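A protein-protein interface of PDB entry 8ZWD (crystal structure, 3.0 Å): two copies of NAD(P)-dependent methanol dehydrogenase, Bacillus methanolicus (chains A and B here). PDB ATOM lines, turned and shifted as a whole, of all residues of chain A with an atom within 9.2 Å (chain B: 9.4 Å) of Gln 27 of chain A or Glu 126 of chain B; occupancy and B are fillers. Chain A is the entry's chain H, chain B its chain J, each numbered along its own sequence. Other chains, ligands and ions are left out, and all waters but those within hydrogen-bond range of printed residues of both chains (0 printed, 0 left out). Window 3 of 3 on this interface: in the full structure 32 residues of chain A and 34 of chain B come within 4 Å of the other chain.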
ATOM      1  N   ALA A  10      11.556 -20.675 -28.226  1.00  0.00           N
ATOM      2  CA  ALA A  10      10.857 -20.872 -26.960  1.00  0.00           C
ATOM      3  C   ALA A  10      11.687 -21.778 -26.064  1.00  0.00           C
ATOM      4  O   ALA A  10      12.019 -22.905 -26.449  1.00  0.00           O
ATOM      5  CB  ALA A  10       9.465 -21.473 -27.180  1.00  0.00           C
ATOM      6  N   GLU A  20       5.268 -28.817 -19.547  1.00  0.00           N
ATOM      7  CA  GLU A  20       4.827 -28.071 -20.716  1.00  0.00           C
ATOM      8  C   GLU A  20       5.091 -28.803 -22.024  1.00  0.00           C
ATOM      9  O   GLU A  20       4.703 -28.291 -23.082  1.00  0.00           O
ATOM     10  CB  GLU A  20       5.492 -26.691 -20.738  1.00  0.00           C
ATOM     11  CG  GLU A  20       5.486 -25.999 -19.384  1.00  0.00           C
ATOM     12  CD  GLU A  20       5.235 -24.504 -19.477  1.00  0.00           C
ATOM     13  OE1 GLU A  20       5.447 -23.919 -20.564  1.00  0.00           O
ATOM     14  OE2 GLU A  20       4.818 -23.911 -18.459  1.00  0.00           O
ATOM     15  N   VAL A  21       5.691 -30.002 -21.976  1.00  0.00           N
ATOM     16  CA  VAL A  21       6.163 -30.654 -23.199  1.00  0.00           C
ATOM     17  C   VAL A  21       5.044 -30.731 -24.234  1.00  0.00           C
ATOM     18  O   VAL A  21       5.185 -30.248 -25.363  1.00  0.00           O
ATOM     19  CB  VAL A  21       6.757 -32.043 -22.892  1.00  0.00           C
ATOM     20  CG1 VAL A  21       5.784 -32.927 -22.128  1.00  0.00           C
ATOM     21  CG2 VAL A  21       7.184 -32.727 -24.178  1.00  0.00           C
ATOM     22  N   GLY A  22       3.901 -31.298 -23.848  1.00  0.00           N
ATOM     23  CA  GLY A  22       2.798 -31.422 -24.786  1.00  0.00           C
ATOM     24  C   GLY A  22       2.149 -30.088 -25.096  1.00  0.00           C
ATOM     25  O   GLY A  22       1.730 -29.843 -26.233  1.00  0.00           O
ATOM     26  N   THR A  23       2.092 -29.196 -24.101  1.00  0.00           N
ATOM     27  CA  THR A  23       1.372 -27.936 -24.238  1.00  0.00           C
ATOM     28  C   THR A  23       1.891 -27.173 -25.448  1.00  0.00           C
ATOM     29  O   THR A  23       1.177 -27.028 -26.451  1.00  0.00           O
ATOM     30  CB  THR A  23       1.504 -27.097 -22.967  1.00  0.00           C
ATOM     31  OG1 THR A  23       2.801 -26.483 -22.915  1.00  0.00           O
ATOM     32  CG2 THR A  23       1.331 -27.974 -21.734  1.00  0.00           C
ATOM     33  N   ARG A  24       3.148 -26.722 -25.371  1.00  0.00           N
ATOM     34  CA  ARG A  24       3.781 -26.031 -26.489  1.00  0.00           C
ATOM     35  C   ARG A  24       3.610 -26.795 -27.790  1.00  0.00           C
ATOM     36  O   ARG A  24       3.461 -26.183 -28.853  1.00  0.00           O
ATOM     37  CB  ARG A  24       5.277 -25.823 -26.214  1.00  0.00           C
ATOM     38  CG  ARG A  24       5.641 -25.567 -24.756  1.00  0.00           C
ATOM     39  CD  ARG A  24       6.687 -24.472 -24.648  1.00  0.00           C
ATOM     40  NE  ARG A  24       6.229 -23.261 -25.317  1.00  0.00           N
ATOM     41  CZ  ARG A  24       5.455 -22.342 -24.757  1.00  0.00           C
ATOM     42  NH1 ARG A  24       5.060 -22.442 -23.498  1.00  0.00           N
ATOM     43  NH2 ARG A  24       5.067 -21.298 -25.479  1.00  0.00           N
ATOM     44  N   LEU A  25       3.605 -28.131 -27.722  1.00  0.00           N
ATOM     45  CA  LEU A  25       3.559 -28.940 -28.936  1.00  0.00           C
ATOM     46  C   LEU A  25       2.305 -28.648 -29.751  1.00  0.00           C
ATOM     47  O   LEU A  25       2.345 -28.660 -30.991  1.00  0.00           O
ATOM     48  CB  LEU A  25       3.636 -30.423 -28.574  1.00  0.00           C
ATOM     49  CG  LEU A  25       4.009 -31.393 -29.696  1.00  0.00           C
ATOM     50  CD1 LEU A  25       5.313 -30.977 -30.358  1.00  0.00           C
ATOM     51  CD2 LEU A  25       4.106 -32.821 -29.171  1.00  0.00           C
ATOM     52  N   LYS A  26       1.183 -28.368 -29.081  1.00  0.00           N
ATOM     53  CA  LYS A  26      -0.009 -28.037 -29.851  1.00  0.00           C
ATOM     54  C   LYS A  26       0.069 -26.628 -30.429  1.00  0.00           C
ATOM     55  O   LYS A  26      -0.441 -26.390 -31.527  1.00  0.00           O
ATOM     56  CB  LYS A  26      -1.266 -28.205 -28.992  1.00  0.00           C
ATOM     57  CG  LYS A  26      -2.562 -28.043 -29.773  1.00  0.00           C
ATOM     58  CD  LYS A  26      -2.679 -29.064 -30.898  1.00  0.00           C
ATOM     59  CE  LYS A  26      -3.948 -28.844 -31.714  1.00  0.00           C
ATOM     60  NZ  LYS A  26      -5.201 -28.964 -30.910  1.00  0.00           N
ATOM     61  N   GLN A  27       0.720 -25.693 -29.726  1.00  0.00           N
ATOM     62  CA  GLN A  27       0.972 -24.375 -30.305  1.00  0.00           C
ATOM     63  C   GLN A  27       1.719 -24.479 -31.629  1.00  0.00           C
ATOM     64  O   GLN A  27       1.523 -23.650 -32.525  1.00  0.00           O
ATOM     65  CB  GLN A  27       1.764 -23.523 -29.324  1.00  0.00           C
ATOM     66  CG  GLN A  27       0.909 -22.728 -28.370  1.00  0.00           C
ATOM     67  CD  GLN A  27       0.925 -21.251 -28.690  1.00  0.00           C
ATOM     68  OE1 GLN A  27       1.126 -20.851 -29.838  1.00  0.00           O
ATOM     69  NE2 GLN A  27       0.725 -20.427 -27.670  1.00  0.00           N
ATOM     70  N   ILE A  28       2.578 -25.491 -31.766  1.00  0.00           N
ATOM     71  CA  ILE A  28       3.282 -25.755 -33.013  1.00  0.00           C
ATOM     72  C   ILE A  28       2.411 -26.539 -33.990  1.00  0.00           C
ATOM     73  O   ILE A  28       2.705 -26.563 -35.192  1.00  0.00           O
ATOM     74  CB  ILE A  28       4.594 -26.489 -32.685  1.00  0.00           C
ATOM     75  CG1 ILE A  28       5.293 -25.773 -31.529  1.00  0.00           C
ATOM     76  CG2 ILE A  28       5.522 -26.540 -33.888  1.00  0.00           C
ATOM     77  CD1 ILE A  28       6.186 -26.660 -30.703  1.00  0.00           C
ATOM     78  N   GLY A  29       1.339 -27.166 -33.507  1.00  0.00           N
ATOM     79  CA  GLY A  29       0.438 -27.899 -34.371  1.00  0.00           C
ATOM     80  C   GLY A  29       0.967 -29.238 -34.824  1.00  0.00           C
ATOM     81  O   GLY A  29       0.671 -29.668 -35.945  1.00  0.00           O
ATOM     82  N   ALA A  30       1.735 -29.917 -33.978  1.00  0.00           N
ATOM     83  CA  ALA A  30       2.417 -31.150 -34.352  1.00  0.00           C
ATOM     84  C   ALA A  30       1.563 -32.342 -33.932  1.00  0.00           C
ATOM     85  O   ALA A  30       1.394 -32.603 -32.737  1.00  0.00           O
ATOM     86  CB  ALA A  30       3.794 -31.192 -33.704  1.00  0.00           C
ATOM     87  N   LYS A  31       1.046 -33.084 -34.917  1.00  0.00           N
ATOM     88  CA  LYS A  31       0.033 -34.095 -34.629  1.00  0.00           C
ATOM     89  C   LYS A  31       0.632 -35.385 -34.075  1.00  0.00           C
ATOM     90  O   LYS A  31      -0.001 -36.052 -33.249  1.00  0.00           O
ATOM     91  CB  LYS A  31      -0.793 -34.394 -35.885  1.00  0.00           C
ATOM     92  CG  LYS A  31      -1.792 -33.306 -36.282  1.00  0.00           C
ATOM     93  CD  LYS A  31      -1.146 -32.208 -37.127  1.00  0.00           C
ATOM     94  CE  LYS A  31      -2.066 -31.002 -37.297  1.00  0.00           C
ATOM     95  NZ  LYS A  31      -1.425 -29.919 -38.100  1.00  0.00           N
ATOM     96  N   ALA A  57      -2.825 -33.612 -24.557  1.00  0.00           N
ATOM     97  CA  ALA A  57      -3.210 -32.432 -25.312  1.00  0.00           C
ATOM     98  C   ALA A  57      -3.509 -32.744 -26.775  1.00  0.00           C
ATOM     99  O   ALA A  57      -3.796 -31.822 -27.544  1.00  0.00           O
ATOM    100  CB  ALA A  57      -2.111 -31.366 -25.216  1.00  0.00           C
ATOM    101  N   VAL A  59      -1.840 -35.509 -29.168  1.00  0.00           N
ATOM    102  CA  VAL A  59      -0.744 -35.802 -30.087  1.00  0.00           C
ATOM    103  C   VAL A  59      -0.368 -37.279 -29.974  1.00  0.00           C
ATOM    104  O   VAL A  59      -0.313 -37.840 -28.874  1.00  0.00           O
ATOM    105  CB  VAL A  59       0.482 -34.898 -29.807  1.00  0.00           C
ATOM    106  CG1 VAL A  59       1.646 -35.241 -30.730  1.00  0.00           C
ATOM    107  CG2 VAL A  59       0.116 -33.416 -29.923  1.00  0.00           C
ATOM    108  N   PRO A 131       9.800 -29.730 -36.604  1.00  0.00           N
ATOM    109  CA  PRO A 131      10.143 -29.077 -35.334  1.00  0.00           C
ATOM    110  C   PRO A 131      10.653 -30.062 -34.295  1.00  0.00           C
ATOM    111  O   PRO A 131      10.150 -31.182 -34.171  1.00  0.00           O
ATOM    112  CB  PRO A 131       8.815 -28.454 -34.893  1.00  0.00           C
ATOM    113  CG  PRO A 131       8.085 -28.229 -36.150  1.00  0.00           C
ATOM    114  CD  PRO A 131       8.423 -29.411 -37.018  1.00  0.00           C
ATOM    115  N   THR A 170      13.388 -26.417 -31.891  1.00  0.00           N
ATOM    116  CA  THR A 170      12.345 -25.400 -31.876  1.00  0.00           C
ATOM    117  C   THR A 170      11.963 -25.025 -30.454  1.00  0.00           C
ATOM    118  O   THR A 170      11.756 -23.843 -30.160  1.00  0.00           O
ATOM    119  CB  THR A 170      11.112 -25.875 -32.652  1.00  0.00           C
ATOM    120  OG1 THR A 170      11.525 -26.381 -33.932  1.00  0.00           O
ATOM    121  CG2 THR A 170      10.139 -24.720 -32.857  1.00  0.00           C
ATOM    122  N   VAL A 171      11.869 -26.003 -29.559  1.00  0.00           N
ATOM    123  CA  VAL A 171      11.569 -25.715 -28.163  1.00  0.00           C
ATOM    124  C   VAL A 171      12.618 -26.385 -27.279  1.00  0.00           C
ATOM    125  O   VAL A 171      12.982 -27.552 -27.492  1.00  0.00           O
ATOM    126  CB  VAL A 171      10.142 -26.173 -27.788  1.00  0.00           C
ATOM    127  CG1 VAL A 171       9.906 -26.048 -26.296  1.00  0.00           C
ATOM    128  CG2 VAL A 171       9.113 -25.347 -28.547  1.00  0.00           C
ATOM    129  N   ASN B   4       9.803 -18.873 -18.825  1.00  0.00           N
ATOM    130  CA  ASN B   4       9.819 -18.986 -20.274  1.00  0.00           C
ATOM    131  C   ASN B   4      10.699 -17.887 -20.851  1.00  0.00           C
ATOM    132  O   ASN B   4      10.745 -16.771 -20.320  1.00  0.00           O
ATOM    133  CB  ASN B   4       8.400 -18.907 -20.847  1.00  0.00           C
ATOM    134  CG  ASN B   4       7.524 -20.059 -20.380  1.00  0.00           C
ATOM    135  OD1 ASN B   4       7.751 -20.626 -19.309  1.00  0.00           O
ATOM    136  ND2 ASN B   4       6.528 -20.423 -21.189  1.00  0.00           N
ATOM    137  N   PHE B   6      11.437 -16.173 -24.554  1.00  0.00           N
ATOM    138  CA  PHE B   6      10.987 -16.043 -25.932  1.00  0.00           C
ATOM    139  C   PHE B   6      11.868 -15.041 -26.660  1.00  0.00           C
ATOM    140  O   PHE B   6      11.977 -13.882 -26.249  1.00  0.00           O
ATOM    141  CB  PHE B   6       9.518 -15.624 -25.981  1.00  0.00           C
ATOM    142  CG  PHE B   6       8.589 -16.615 -25.345  1.00  0.00           C
ATOM    143  CD1 PHE B   6       8.849 -17.977 -25.430  1.00  0.00           C
ATOM    144  CD2 PHE B   6       7.467 -16.192 -24.648  1.00  0.00           C
ATOM    145  CE1 PHE B   6       7.999 -18.899 -24.842  1.00  0.00           C
ATOM    146  CE2 PHE B   6       6.615 -17.110 -24.054  1.00  0.00           C
ATOM    147  CZ  PHE B   6       6.882 -18.465 -24.152  1.00  0.00           C
ATOM    148  N   LEU B 108      -1.534  -9.628 -36.222  1.00  0.00           N
ATOM    149  CA  LEU B 108      -2.045 -10.444 -35.164  1.00  0.00           C
ATOM    150  C   LEU B 108      -3.463 -10.605 -35.590  1.00  0.00           C
ATOM    151  O   LEU B 108      -3.951 -11.723 -35.715  1.00  0.00           O
ATOM    152  CB  LEU B 108      -1.999  -9.698 -33.838  1.00  0.00           C
ATOM    153  CG  LEU B 108      -2.643 -10.298 -32.590  1.00  0.00           C
ATOM    154  CD1 LEU B 108      -2.073 -11.671 -32.280  1.00  0.00           C
ATOM    155  CD2 LEU B 108      -2.441  -9.362 -31.412  1.00  0.00           C
ATOM    156  N   ALA B 111      -7.879 -12.242 -37.600  1.00  0.00           N
ATOM    157  CA  ALA B 111      -8.877 -13.023 -36.909  1.00  0.00           C
ATOM    158  C   ALA B 111     -10.192 -12.277 -36.950  1.00  0.00           C
ATOM    159  O   ALA B 111     -10.271 -11.183 -37.499  1.00  0.00           O
ATOM    160  CB  ALA B 111      -8.437 -13.224 -35.479  1.00  0.00           C
ATOM    161  N   ASN B 123      -1.943 -12.035 -23.349  1.00  0.00           N
ATOM    162  CA  ASN B 123      -2.866 -12.842 -24.132  1.00  0.00           C
ATOM    163  C   ASN B 123      -2.243 -14.189 -24.466  1.00  0.00           C
ATOM    164  O   ASN B 123      -1.020 -14.358 -24.444  1.00  0.00           O
ATOM    165  CB  ASN B 123      -3.260 -12.140 -25.435  1.00  0.00           C
ATOM    166  CG  ASN B 123      -3.620 -10.686 -25.231  1.00  0.00           C
ATOM    167  OD1 ASN B 123      -2.896  -9.787 -25.659  1.00  0.00           O
ATOM    168  ND2 ASN B 123      -4.751 -10.445 -24.578  1.00  0.00           N
ATOM    169  N   SER B 124      -3.108 -15.145 -24.790  1.00  0.00           N
ATOM    170  CA  SER B 124      -2.686 -16.464 -25.231  1.00  0.00           C
ATOM    171  C   SER B 124      -2.971 -16.670 -26.708  1.00  0.00           C
ATOM    172  O   SER B 124      -2.125 -17.217 -27.430  1.00  0.00           O
ATOM    173  CB  SER B 124      -3.377 -17.554 -24.399  1.00  0.00           C
ATOM    174  OG  SER B 124      -4.668 -17.838 -24.912  1.00  0.00           O
ATOM    175  N   VAL B 125      -4.168 -16.277 -27.154  1.00  0.00           N
ATOM    176  CA  VAL B 125      -4.517 -16.148 -28.568  1.00  0.00           C
ATOM    177  C   VAL B 125      -4.794 -17.507 -29.215  1.00  0.00           C
ATOM    178  O   VAL B 125      -5.893 -17.738 -29.726  1.00  0.00           O
ATOM    179  CB  VAL B 125      -3.428 -15.355 -29.321  1.00  0.00           C
ATOM    180  CG1 VAL B 125      -3.601 -15.472 -30.800  1.00  0.00           C
ATOM    181  CG2 VAL B 125      -3.462 -13.891 -28.885  1.00  0.00           C
ATOM    182  N   GLU B 126      -3.809 -18.409 -29.211  1.00  0.00           N
ATOM    183  CA  GLU B 126      -3.974 -19.800 -29.667  1.00  0.00           C
ATOM    184  C   GLU B 126      -4.513 -19.892 -31.092  1.00  0.00           C
ATOM    185  O   GLU B 126      -5.367 -20.729 -31.394  1.00  0.00           O
ATOM    186  CB  GLU B 126      -4.880 -20.591 -28.717  1.00  0.00           C
ATOM    187  CG  GLU B 126      -4.624 -20.354 -27.240  1.00  0.00           C
ATOM    188  CD  GLU B 126      -3.280 -20.883 -26.776  1.00  0.00           C
ATOM    189  OE1 GLU B 126      -2.980 -22.066 -27.044  1.00  0.00           O
ATOM    190  OE2 GLU B 126      -2.522 -20.116 -26.142  1.00  0.00           O
ATOM    191  N   LYS B 127      -4.006 -19.036 -31.979  1.00  0.00           N
ATOM    192  CA  LYS B 127      -4.381 -19.078 -33.390  1.00  0.00           C
ATOM    193  C   LYS B 127      -3.226 -18.553 -34.229  1.00  0.00           C
ATOM    194  O   LYS B 127      -2.601 -17.550 -33.866  1.00  0.00           O
ATOM    195  CB  LYS B 127      -5.654 -18.255 -33.665  1.00  0.00           C
ATOM    196  CG  LYS B 127      -5.572 -16.789 -33.283  1.00  0.00           C
ATOM    197  CD  LYS B 127      -6.894 -16.071 -33.492  1.00  0.00           C
ATOM    198  CE  LYS B 127      -7.889 -16.366 -32.382  1.00  0.00           C
ATOM    199  NZ  LYS B 127      -9.151 -15.586 -32.539  1.00  0.00           N
ATOM    200  N   PRO B 128      -2.933 -19.199 -35.344  1.00  0.00           N
ATOM    201  CA  PRO B 128      -1.708 -18.879 -36.098  1.00  0.00           C
ATOM    202  C   PRO B 128      -1.687 -17.443 -36.603  1.00  0.00           C
ATOM    203  O   PRO B 128      -2.676 -16.931 -37.137  1.00  0.00           O
ATOM    204  CB  PRO B 128      -1.743 -19.883 -37.268  1.00  0.00           C
ATOM    205  CG  PRO B 128      -3.128 -20.461 -37.259  1.00  0.00           C
ATOM    206  CD  PRO B 128      -3.626 -20.391 -35.875  1.00  0.00           C
ATOM    207  N   VAL B 129      -0.540 -16.799 -36.425  1.00  0.00           N
ATOM    208  CA  VAL B 129      -0.297 -15.472 -36.971  1.00  0.00           C
ATOM    209  C   VAL B 129       0.765 -15.586 -38.056  1.00  0.00           C
ATOM    210  O   VAL B 129       1.233 -16.687 -38.366  1.00  0.00           O
ATOM    211  CB  VAL B 129       0.138 -14.480 -35.877  1.00  0.00           C
ATOM    212  CG1 VAL B 129      -0.916 -14.402 -34.785  1.00  0.00           C
ATOM    213  CG2 VAL B 129       1.478 -14.905 -35.311  1.00  0.00           C
ATOM    214  N   ASP B 164       1.636 -10.931 -26.193  1.00  0.00           N
ATOM    215  CA  ASP B 164       1.316 -12.290 -26.613  1.00  0.00           C
ATOM    216  C   ASP B 164       2.587 -12.951 -27.127  1.00  0.00           C
ATOM    217  O   ASP B 164       3.499 -12.277 -27.610  1.00  0.00           O
ATOM    218  CB  ASP B 164       0.222 -12.319 -27.690  1.00  0.00           C
ATOM    219  CG  ASP B 164       0.146 -13.659 -28.411  1.00  0.00           C
ATOM    220  OD1 ASP B 164       0.103 -14.706 -27.726  1.00  0.00           O
ATOM    221  OD2 ASP B 164       0.142 -13.667 -29.661  1.00  0.00           O
ATOM    222  N   GLU B 165       2.640 -14.280 -27.012  1.00  0.00           N
ATOM    223  CA  GLU B 165       3.830 -14.999 -27.450  1.00  0.00           C
ATOM    224  C   GLU B 165       4.011 -14.926 -28.963  1.00  0.00           C
ATOM    225  O   GLU B 165       5.140 -14.781 -29.449  1.00  0.00           O
ATOM    226  CB  GLU B 165       3.768 -16.453 -26.993  1.00  0.00           C
ATOM    227  CG  GLU B 165       4.925 -17.297 -27.503  1.00  0.00           C
ATOM    228  CD  GLU B 165       4.901 -18.707 -26.957  1.00  0.00           C
ATOM    229  OE1 GLU B 165       4.057 -18.987 -26.076  1.00  0.00           O
ATOM    230  OE2 GLU B 165       5.724 -19.536 -27.406  1.00  0.00           O
ATOM    231  N   LYS B 166       2.918 -15.017 -29.725  1.00  0.00           N
ATOM    232  CA  LYS B 166       3.043 -15.178 -31.168  1.00  0.00           C
ATOM    233  C   LYS B 166       3.456 -13.894 -31.882  1.00  0.00           C
ATOM    234  O   LYS B 166       3.797 -13.952 -33.068  1.00  0.00           O
ATOM    235  CB  LYS B 166       1.728 -15.708 -31.745  1.00  0.00           C
ATOM    236  CG  LYS B 166       1.482 -17.187 -31.443  1.00  0.00           C
ATOM    237  CD  LYS B 166       2.676 -18.058 -31.849  1.00  0.00           C
ATOM    238  CE  LYS B 166       2.781 -18.231 -33.365  1.00  0.00           C
ATOM    239  NZ  LYS B 166       1.809 -19.221 -33.924  1.00  0.00           N
ATOM    240  N   ILE B 167       3.448 -12.745 -31.202  1.00  0.00           N
ATOM    241  CA  ILE B 167       3.864 -11.501 -31.850  1.00  0.00           C
ATOM    242  C   ILE B 167       5.359 -11.283 -31.631  1.00  0.00           C
ATOM    243  O   ILE B 167       5.891 -10.205 -31.925  1.00  0.00           O
ATOM    244  CB  ILE B 167       3.050 -10.277 -31.372  1.00  0.00           C
ATOM    245  CG1 ILE B 167       2.808 -10.309 -29.865  1.00  0.00           C
ATOM    246  CG2 ILE B 167       1.737 -10.166 -32.121  1.00  0.00           C
ATOM    247  CD1 ILE B 167       2.321  -8.993 -29.313  1.00  0.00           C
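Among the printed residues, merely in contact across the chains: Gln 27 of chain A with Glu 126 of chain B (3.6 Å), Arg 24 of chain A with Phe 6 of chain B (3.6 Å), Glu 20 of chain A with Asn 4 of chain B (3.7 Å), Ala 10 of chain A with Phe 6 of chain B (3.8 Å), Gln 27 of chain A with Lys 166 of chain B (3.8 Å) and Gln 27 of chain A with Glu 165 of chain B (3.96 Å).
Of the 15 printed residues of chain B, 5 touch a printed residue of chain A. Printed residues of chain B that touch a printed residue of chain A: Asn 4, Phe 6, Glu 126, Glu 165 and Lys 166. Of the 18 printed residues of chain A, 4 touch a printed residue of chain B. Hydrophobic or aromatic side chains of chain A within 4 Å of the printed part of chain B: Ala 10. Along chain A the printed residues that touch a printed residue of chain B span positions 10 to 27. Among the printed residues, Asp or Glu carboxylates within 4 Å of a Lys or Arg side-chain nitrogen of the other chain: Arg 24 of chain A with Glu 165 of chain B.
Printed residues of chain B within 4 Å of Ala 10 of chain A: Phe 6 (3.8 Å). Leu 25 of chain A touches none of the printed residues of chain B. Of chain B, only Glu 126, Glu 165 and Lys 166 come within 4 Å of Gln 27 of chain A. No residue of chain B comes within 4 Å of Ile 28 of chain A. Of the printed residues of chain A, Phe 6 of chain B touches Ala 10 and Arg 24. No residue of chain A comes within 4 Å of Val 125 of chain B. Of chain A, only Gln 27 comes within 4 Å of Glu 126 of chain B. Pro 128 of chain B touches none of the printed residues of chain A. The nearest residue of chain B that does not touch Gln 27 of chain A is Ser 124 of chain B (4.3 Å).
The side-chain hydroxyl (OG1) of Thr 23 of chain A is in hydrogen-bond range of the backbone carbonyl oxygen (O) of Glu 20 of chain A, at 2.6 Å. OE2 of Glu 126 of chain B lies close to OG of Ser 124 of chain B, at 3.4 Å. The side-chain carboxylate (OD2) of Asp 164 of chain B sits at hydrogen-bond distance from the backbone NH (N) of Lys 166 of chain B. OE1 of Glu 20 of chain A lies within salt-bridge range of NH1 of Arg 24 of chain A (3.3 Å).
No position is printed for both chains.
The guanidinium group of Arg 24 of chain A is in salt-bridge range of the side-chain carboxylate of Glu 165 of chain B (2.6 Å). The guanidinium group (NH1) of Arg 24 of chain A sits close to the side-chain amide nitrogen (ND2) of Asn 4 of chain B, at 3.4 Å.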
